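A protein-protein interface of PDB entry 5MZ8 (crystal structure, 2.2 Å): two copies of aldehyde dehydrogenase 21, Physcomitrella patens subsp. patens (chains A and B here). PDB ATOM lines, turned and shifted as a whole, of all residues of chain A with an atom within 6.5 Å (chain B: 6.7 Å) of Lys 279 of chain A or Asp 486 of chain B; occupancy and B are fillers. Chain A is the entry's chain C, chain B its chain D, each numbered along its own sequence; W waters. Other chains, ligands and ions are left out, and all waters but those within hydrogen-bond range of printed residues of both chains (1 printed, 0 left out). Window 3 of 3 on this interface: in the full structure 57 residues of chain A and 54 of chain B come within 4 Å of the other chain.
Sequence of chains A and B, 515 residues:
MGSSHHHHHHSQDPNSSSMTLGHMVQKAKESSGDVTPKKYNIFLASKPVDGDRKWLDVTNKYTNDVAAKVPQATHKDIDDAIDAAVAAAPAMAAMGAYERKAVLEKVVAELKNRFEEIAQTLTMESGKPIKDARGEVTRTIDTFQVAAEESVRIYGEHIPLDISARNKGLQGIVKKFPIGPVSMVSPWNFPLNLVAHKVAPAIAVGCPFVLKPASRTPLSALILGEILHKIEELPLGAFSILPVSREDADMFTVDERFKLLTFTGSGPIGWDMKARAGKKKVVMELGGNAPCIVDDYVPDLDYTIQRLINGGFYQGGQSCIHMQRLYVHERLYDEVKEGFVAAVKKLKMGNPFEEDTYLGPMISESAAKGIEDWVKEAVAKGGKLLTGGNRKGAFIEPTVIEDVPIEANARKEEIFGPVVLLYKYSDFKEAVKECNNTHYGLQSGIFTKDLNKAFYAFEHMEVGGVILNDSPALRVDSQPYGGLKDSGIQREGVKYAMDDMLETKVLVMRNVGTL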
ATOM      1  N   GLU A 256     -10.561   3.695  -1.505  1.00  0.00           N
ATOM      2  CA  GLU A 256     -10.765   3.433  -2.926  1.00  0.00           C
ATOM      3  C   GLU A 256     -11.168   2.011  -3.245  1.00  0.00           C
ATOM      4  O   GLU A 256     -11.713   1.784  -4.321  1.00  0.00           O
ATOM      5  CB  GLU A 256      -9.535   3.828  -3.757  1.00  0.00           C
ATOM      6  CG  GLU A 256      -9.346   5.331  -3.884  1.00  0.00           C
ATOM      7  CD  GLU A 256      -7.945   5.818  -4.212  1.00  0.00           C
ATOM      8  OE1 GLU A 256      -7.507   6.821  -3.600  1.00  0.00           O
ATOM      9  OE2 GLU A 256      -7.295   5.220  -5.102  1.00  0.00           O
ATOM     10  N   PHE A 258     -13.575   0.324  -1.813  1.00  0.00           N
ATOM     11  CA  PHE A 258     -15.038   0.261  -1.766  1.00  0.00           C
ATOM     12  C   PHE A 258     -15.584   0.880  -3.051  1.00  0.00           C
ATOM     13  O   PHE A 258     -15.081   1.912  -3.516  1.00  0.00           O
ATOM     14  CB  PHE A 258     -15.598   1.049  -0.582  1.00  0.00           C
ATOM     15  CG  PHE A 258     -15.338   0.529   0.803  1.00  0.00           C
ATOM     16  CD1 PHE A 258     -15.882  -0.682   1.219  1.00  0.00           C
ATOM     17  CD2 PHE A 258     -14.654   1.302   1.734  1.00  0.00           C
ATOM     18  CE1 PHE A 258     -15.706  -1.129   2.527  1.00  0.00           C
ATOM     19  CE2 PHE A 258     -14.472   0.848   3.042  1.00  0.00           C
ATOM     20  CZ  PHE A 258     -15.006  -0.358   3.434  1.00  0.00           C
ATOM     21  N   LYS A 259     -16.623   0.264  -3.608  1.00  0.00           N
ATOM     22  CA  LYS A 259     -17.274   0.720  -4.835  1.00  0.00           C
ATOM     23  C   LYS A 259     -18.527   1.541  -4.532  1.00  0.00           C
ATOM     24  O   LYS A 259     -19.012   2.281  -5.382  1.00  0.00           O
ATOM     25  CB  LYS A 259     -17.605  -0.491  -5.726  1.00  0.00           C
ATOM     26  CG  LYS A 259     -16.377  -1.323  -6.178  1.00  0.00           C
ATOM     27  CD  LYS A 259     -15.327  -0.553  -7.019  1.00  0.00           C
ATOM     28  CE  LYS A 259     -15.627  -0.560  -8.513  1.00  0.00           C
ATOM     29  NZ  LYS A 259     -14.592   0.123  -9.340  1.00  0.00           N
ATOM     30  N   ALA A 277     -15.874  11.242  -0.515  1.00  0.00           N
ATOM     31  CA  ALA A 277     -15.940   9.831  -0.919  1.00  0.00           C
ATOM     32  C   ALA A 277     -14.992   9.400  -2.059  1.00  0.00           C
ATOM     33  O   ALA A 277     -14.632   8.227  -2.141  1.00  0.00           O
ATOM     34  CB  ALA A 277     -17.370   9.470  -1.289  1.00  0.00           C
ATOM     35  N   GLY A 278     -14.618  10.335  -2.928  1.00  0.00           N
ATOM     36  CA  GLY A 278     -13.770  10.035  -4.079  1.00  0.00           C
ATOM     37  C   GLY A 278     -14.601   9.523  -5.243  1.00  0.00           C
ATOM     38  O   GLY A 278     -15.677  10.061  -5.512  1.00  0.00           O
ATOM     39  N   LYS A 279     -14.141   8.438  -5.898  1.00  0.00           N
ATOM     40  CA  LYS A 279     -14.753   7.890  -7.116  1.00  0.00           C
ATOM     41  C   LYS A 279     -15.976   6.987  -6.899  1.00  0.00           C
ATOM     42  O   LYS A 279     -16.774   6.839  -7.822  1.00  0.00           O
ATOM     43  CB  LYS A 279     -13.701   7.163  -7.979  1.00  0.00           C
ATOM     44  CG  LYS A 279     -12.528   8.047  -8.352  1.00  0.00           C
ATOM     45  CD  LYS A 279     -11.577   7.356  -9.305  1.00  0.00           C
ATOM     46  CE  LYS A 279     -10.290   8.132  -9.412  1.00  0.00           C
ATOM     47  NZ  LYS A 279      -9.447   7.639 -10.522  1.00  0.00           N
ATOM     48  N   LYS A 280     -16.142   6.403  -5.700  1.00  0.00           N
ATOM     49  CA  LYS A 280     -17.270   5.518  -5.402  1.00  0.00           C
ATOM     50  C   LYS A 280     -18.634   6.201  -5.509  1.00  0.00           C
ATOM     51  O   LYS A 280     -18.728   7.420  -5.372  1.00  0.00           O
ATOM     52  CB  LYS A 280     -17.121   4.876  -4.013  1.00  0.00           C
ATOM     53  CG  LYS A 280     -17.075   5.872  -2.844  1.00  0.00           C
ATOM     54  CD  LYS A 280     -16.977   5.177  -1.493  1.00  0.00           C
ATOM     55  CE  LYS A 280     -15.610   4.612  -1.166  1.00  0.00           C
ATOM     56  NZ  LYS A 280     -14.549   5.651  -1.117  1.00  0.00           N
ATOM     57  N   LYS A 281     -19.689   5.392  -5.716  1.00  0.00           N
ATOM     58  CA  LYS A 281     -21.086   5.809  -5.731  1.00  0.00           C
ATOM     59  C   LYS A 281     -21.494   6.013  -4.271  1.00  0.00           C
ATOM     60  O   LYS A 281     -20.923   5.392  -3.377  1.00  0.00           O
ATOM     61  CB  LYS A 281     -21.975   4.741  -6.404  1.00  0.00           C
ATOM     62  CG  LYS A 281     -21.838   4.703  -7.923  1.00  0.00           C
ATOM     63  CD  LYS A 281     -22.913   3.842  -8.559  1.00  0.00           C
ATOM     64  CE  LYS A 281     -22.760   3.809 -10.051  1.00  0.00           C
ATOM     65  NZ  LYS A 281     -23.880   3.086 -10.707  1.00  0.00           N
ATOM     66  N   GLY B 267     -11.413  12.361 -17.741  1.00  0.00           N
ATOM     67  CA  GLY B 267     -11.467  11.693 -16.444  1.00  0.00           C
ATOM     68  C   GLY B 267     -10.976  12.547 -15.285  1.00  0.00           C
ATOM     69  O   GLY B 267     -11.755  12.791 -14.362  1.00  0.00           O
ATOM     70  N   TRP B 271     -13.695  13.502 -12.412  1.00  0.00           N
ATOM     71  CA  TRP B 271     -13.548  13.072 -11.020  1.00  0.00           C
ATOM     72  C   TRP B 271     -13.415  14.260 -10.045  1.00  0.00           C
ATOM     73  O   TRP B 271     -14.021  14.232  -8.971  1.00  0.00           O
ATOM     74  CB  TRP B 271     -12.409  12.047 -10.861  1.00  0.00           C
ATOM     75  CG  TRP B 271     -12.670  10.742 -11.574  1.00  0.00           C
ATOM     76  CD1 TRP B 271     -11.903  10.180 -12.548  1.00  0.00           C
ATOM     77  CD2 TRP B 271     -13.795   9.849 -11.384  1.00  0.00           C
ATOM     78  NE1 TRP B 271     -12.468   9.001 -12.981  1.00  0.00           N
ATOM     79  CE2 TRP B 271     -13.623   8.767 -12.277  1.00  0.00           C
ATOM     80  CE3 TRP B 271     -14.932   9.858 -10.539  1.00  0.00           C
ATOM     81  CZ2 TRP B 271     -14.547   7.710 -12.366  1.00  0.00           C
ATOM     82  CZ3 TRP B 271     -15.862   8.825 -10.649  1.00  0.00           C
ATOM     83  CH2 TRP B 271     -15.658   7.759 -11.542  1.00  0.00           C
ATOM     84  N   LYS B 274     -16.950  15.774  -9.696  1.00  0.00           N
ATOM     85  CA  LYS B 274     -17.738  14.905  -8.816  1.00  0.00           C
ATOM     86  C   LYS B 274     -17.432  15.240  -7.345  1.00  0.00           C
ATOM     87  O   LYS B 274     -18.363  15.344  -6.549  1.00  0.00           O
ATOM     88  CB  LYS B 274     -17.427  13.423  -9.106  1.00  0.00           C
ATOM     89  CG  LYS B 274     -18.276  12.439  -8.305  1.00  0.00           C
ATOM     90  CD  LYS B 274     -17.832  11.004  -8.503  1.00  0.00           C
ATOM     91  CE  LYS B 274     -18.691  10.012  -7.736  1.00  0.00           C
ATOM     92  NZ  LYS B 274     -18.355   9.990  -6.283  1.00  0.00           N
ATOM     93  N   LEU B 286     -16.645   9.150 -19.086  1.00  0.00           N
ATOM     94  CA  LEU B 286     -15.235   9.530 -19.201  1.00  0.00           C
ATOM     95  C   LEU B 286     -14.476   8.671 -20.225  1.00  0.00           C
ATOM     96  O   LEU B 286     -15.103   8.046 -21.089  1.00  0.00           O
ATOM     97  CB  LEU B 286     -14.535   9.573 -17.812  1.00  0.00           C
ATOM     98  CG  LEU B 286     -15.295  10.295 -16.653  1.00  0.00           C
ATOM     99  CD1 LEU B 286     -14.635  10.045 -15.323  1.00  0.00           C
ATOM    100  CD2 LEU B 286     -15.404  11.793 -16.878  1.00  0.00           C
ATOM    101  N   GLY B 287     -13.146   8.699 -20.169  1.00  0.00           N
ATOM    102  CA  GLY B 287     -12.300   7.980 -21.117  1.00  0.00           C
ATOM    103  C   GLY B 287     -12.384   6.464 -21.100  1.00  0.00           C
ATOM    104  O   GLY B 287     -13.153   5.878 -20.334  1.00  0.00           O
ATOM    105  N   GLY B 288     -11.577   5.840 -21.952  1.00  0.00           N
ATOM    106  CA  GLY B 288     -11.456   4.396 -22.056  1.00  0.00           C
ATOM    107  C   GLY B 288     -10.128   3.969 -22.650  1.00  0.00           C
ATOM    108  O   GLY B 288      -9.352   4.796 -23.138  1.00  0.00           O
ATOM    109  N   HIS B 439      -7.227   0.602 -15.786  1.00  0.00           N
ATOM    110  CA  HIS B 439      -7.979   1.379 -14.789  1.00  0.00           C
ATOM    111  C   HIS B 439      -9.246   1.956 -15.410  1.00  0.00           C
ATOM    112  O   HIS B 439     -10.049   2.578 -14.727  1.00  0.00           O
ATOM    113  CB  HIS B 439      -7.115   2.462 -14.117  1.00  0.00           C
ATOM    114  CG  HIS B 439      -6.432   3.393 -15.065  1.00  0.00           C
ATOM    115  ND1 HIS B 439      -5.280   3.018 -15.743  1.00  0.00           N
ATOM    116  CD2 HIS B 439      -6.726   4.678 -15.381  1.00  0.00           C
ATOM    117  CE1 HIS B 439      -4.927   4.076 -16.460  1.00  0.00           C
ATOM    118  NE2 HIS B 439      -5.760   5.102 -16.265  1.00  0.00           N
ATOM    119  N   TYR B 440      -9.424   1.717 -16.709  1.00  0.00           N
ATOM    120  CA  TYR B 440     -10.606   2.111 -17.470  1.00  0.00           C
ATOM    121  C   TYR B 440     -11.529   0.881 -17.557  1.00  0.00           C
ATOM    122  O   TYR B 440     -11.113  -0.225 -17.227  1.00  0.00           O
ATOM    123  CB  TYR B 440     -10.194   2.588 -18.873  1.00  0.00           C
ATOM    124  CG  TYR B 440      -9.287   3.800 -18.898  1.00  0.00           C
ATOM    125  CD1 TYR B 440      -9.801   5.085 -18.728  1.00  0.00           C
ATOM    126  CD2 TYR B 440      -7.936   3.677 -19.209  1.00  0.00           C
ATOM    127  CE1 TYR B 440      -8.982   6.214 -18.823  1.00  0.00           C
ATOM    128  CE2 TYR B 440      -7.109   4.797 -19.315  1.00  0.00           C
ATOM    129  CZ  TYR B 440      -7.633   6.066 -19.112  1.00  0.00           C
ATOM    130  OH  TYR B 440      -6.817   7.173 -19.197  1.00  0.00           O
ATOM    131  N   GLY B 441     -12.761   1.080 -17.994  1.00  0.00           N
ATOM    132  CA  GLY B 441     -13.721  -0.009 -18.135  1.00  0.00           C
ATOM    133  C   GLY B 441     -14.996   0.401 -18.837  1.00  0.00           C
ATOM    134  O   GLY B 441     -16.081   0.204 -18.295  1.00  0.00           O
ATOM    135  N   GLY B 483     -19.465   3.211 -18.218  1.00  0.00           N
ATOM    136  CA  GLY B 483     -18.426   2.311 -17.756  1.00  0.00           C
ATOM    137  C   GLY B 483     -18.278   2.067 -16.286  1.00  0.00           C
ATOM    138  O   GLY B 483     -19.063   2.541 -15.458  1.00  0.00           O
ATOM    139  N   LEU B 484     -17.242   1.298 -15.984  1.00  0.00           N
ATOM    140  CA  LEU B 484     -16.809   0.930 -14.636  1.00  0.00           C
ATOM    141  C   LEU B 484     -15.450   1.560 -14.440  1.00  0.00           C
ATOM    142  O   LEU B 484     -14.886   2.116 -15.390  1.00  0.00           O
ATOM    143  CB  LEU B 484     -16.678  -0.601 -14.527  1.00  0.00           C
ATOM    144  CG  LEU B 484     -17.915  -1.433 -14.839  1.00  0.00           C
ATOM    145  CD1 LEU B 484     -17.634  -2.882 -14.590  1.00  0.00           C
ATOM    146  CD2 LEU B 484     -19.099  -1.001 -14.002  1.00  0.00           C
ATOM    147  N   LYS B 485     -14.902   1.457 -13.218  1.00  0.00           N
ATOM    148  CA  LYS B 485     -13.583   1.983 -12.854  1.00  0.00           C
ATOM    149  C   LYS B 485     -13.450   3.494 -13.171  1.00  0.00           C
ATOM    150  O   LYS B 485     -14.356   4.251 -12.817  1.00  0.00           O
ATOM    151  CB  LYS B 485     -12.461   1.131 -13.475  1.00  0.00           C
ATOM    152  CG  LYS B 485     -12.585  -0.371 -13.232  1.00  0.00           C
ATOM    153  CD  LYS B 485     -11.438  -1.078 -13.911  1.00  0.00           C
ATOM    154  CE  LYS B 485     -11.597  -2.562 -13.940  1.00  0.00           C
ATOM    155  NZ  LYS B 485     -10.524  -3.175 -14.761  1.00  0.00           N
ATOM    156  N   ASP B 486     -12.362   3.934 -13.853  1.00  0.00           N
ATOM    157  CA  ASP B 486     -12.140   5.356 -14.168  1.00  0.00           C
ATOM    158  C   ASP B 486     -12.944   5.865 -15.360  1.00  0.00           C
ATOM    159  O   ASP B 486     -12.911   7.063 -15.646  1.00  0.00           O
ATOM    160  CB  ASP B 486     -10.648   5.666 -14.353  1.00  0.00           C
ATOM    161  CG  ASP B 486      -9.801   5.556 -13.093  1.00  0.00           C
ATOM    162  OD1 ASP B 486     -10.338   5.156 -12.043  1.00  0.00           O
ATOM    163  OD2 ASP B 486      -8.605   5.874 -13.159  1.00  0.00           O
ATOM    164  N   SER B 487     -13.693   4.975 -16.024  1.00  0.00           N
ATOM    165  CA  SER B 487     -14.502   5.335 -17.200  1.00  0.00           C
ATOM    166  C   SER B 487     -15.785   6.106 -16.860  1.00  0.00           C
ATOM    167  O   SER B 487     -16.444   6.584 -17.765  1.00  0.00           O
ATOM    168  CB  SER B 487     -14.800   4.109 -18.058  1.00  0.00           C
ATOM    169  OG  SER B 487     -13.611   3.601 -18.643  1.00  0.00           O
ATOM    170  N   GLY B 488     -16.114   6.251 -15.583  1.00  0.00           N
ATOM    171  CA  GLY B 488     -17.265   7.044 -15.178  1.00  0.00           C
ATOM    172  C   GLY B 488     -18.239   6.369 -14.246  1.00  0.00           C
ATOM    173  O   GLY B 488     -17.956   5.298 -13.710  1.00  0.00           O
ATOM    174  N   ILE B 489     -19.398   7.020 -14.038  1.00  0.00           N
ATOM    175  CA  ILE B 489     -20.513   6.533 -13.221  1.00  0.00           C
ATOM    176  C   ILE B 489     -21.851   6.731 -13.961  1.00  0.00           C
ATOM    177  O   ILE B 489     -22.042   7.752 -14.609  1.00  0.00           O
ATOM    178  CB  ILE B 489     -20.541   7.069 -11.759  1.00  0.00           C
ATOM    179  CG1 ILE B 489     -20.527   8.611 -11.686  1.00  0.00           C
ATOM    180  CG2 ILE B 489     -19.407   6.449 -10.904  1.00  0.00           C
ATOM    181  CD1 ILE B 489     -21.202   9.154 -10.467  1.00  0.00           C
HETATM  182  O   HOH W   1     -13.948  12.076  -7.351  1.00  0.00           O
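No position is printed for both chains.
Of the 5 pairs that touch across the chains among the printed residues, none has its exchanged pair printed and touching as well.
Water W1 bridges the backbone carbonyl oxygen (O) of Trp 271 of chain B (2.7 Å) and the backbone carbonyl oxygen (O) of Gly 278 of chain A (3.2 Å).
The backbone carbonyl oxygen (O) of Gly 278 of chain A lies within hydrogen-bond range of the side-chain amino group (NZ) of Lys 274 of chain B, at 2.8 Å.
NZ of Lys 279 of chain A lies within salt-bridge range of OD1 of Asp 486 of chain B, 3.0 Å away.
O of Lys 280 of chain A lies within hydrogen-bond range of NZ of Lys 274 of chain B, 2.8 Å away.
Of chain B, only Trp 271, Lys 274 and Asp 486 come within 4 Å of Lys 279 of chain A.
Of the printed residues of chain A, Asp 486 of chain B touches Lys 279.
Of the printed residues of chain B, Lys 280 of chain A touches Lys 274 (2.8 Å).
Printed residues of chain A within 4 Å of Lys 274 of chain B: Gly 278, Lys 279 and Lys 280.
Printed residues of chain A within 4 Å of Trp 271 of chain B: Lys 279 (3.6 Å).
The nearest printed residue of chain B that does not touch Lys 280 of chain A is Ile 489 of chain B (5.5 Å).
Lys 279 of chain A touches Trp 271 of chain B.
CE of Lys 274 of chain B touches O of Lys 279 of chain A (3.7 Å).
Of the 8 printed residues of chain A, 3 touch a printed residue of chain B.
Printed residues of chain A that touch a printed residue of chain B: Gly 278, Lys 279 and Lys 280.
Of the 16 printed residues of chain B, 3 touch a printed residue of chain A.
Printed residues of chain B that touch a printed residue of chain A: Trp 271, Lys 274 and Asp 486.
Hydrophobic or aromatic side chains of chain B that line the printed part of chain A: Trp 271.
Among the printed residues, Asp or Glu carboxylates within 4 Å of a Lys or Arg side-chain nitrogen of the other chain: Lys 279 of chain A with Asp 486 of chain B.
O of Ala 277 of chain A lies within hydrogen-bond range of NZ of Lys 280 of chain A, at 2.8 Å.
The backbone carbonyl oxygen (O) of Asp 486 of chain B is in hydrogen-bond range of the indole nitrogen (NE1) of Trp 271 of chain B, at 3.3 Å.
The backbone carbonyl oxygen (O) of His 439 of chain B is in hydrogen-bond range of the backbone NH (N) of Asp 486 of chain B (2.8 Å).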
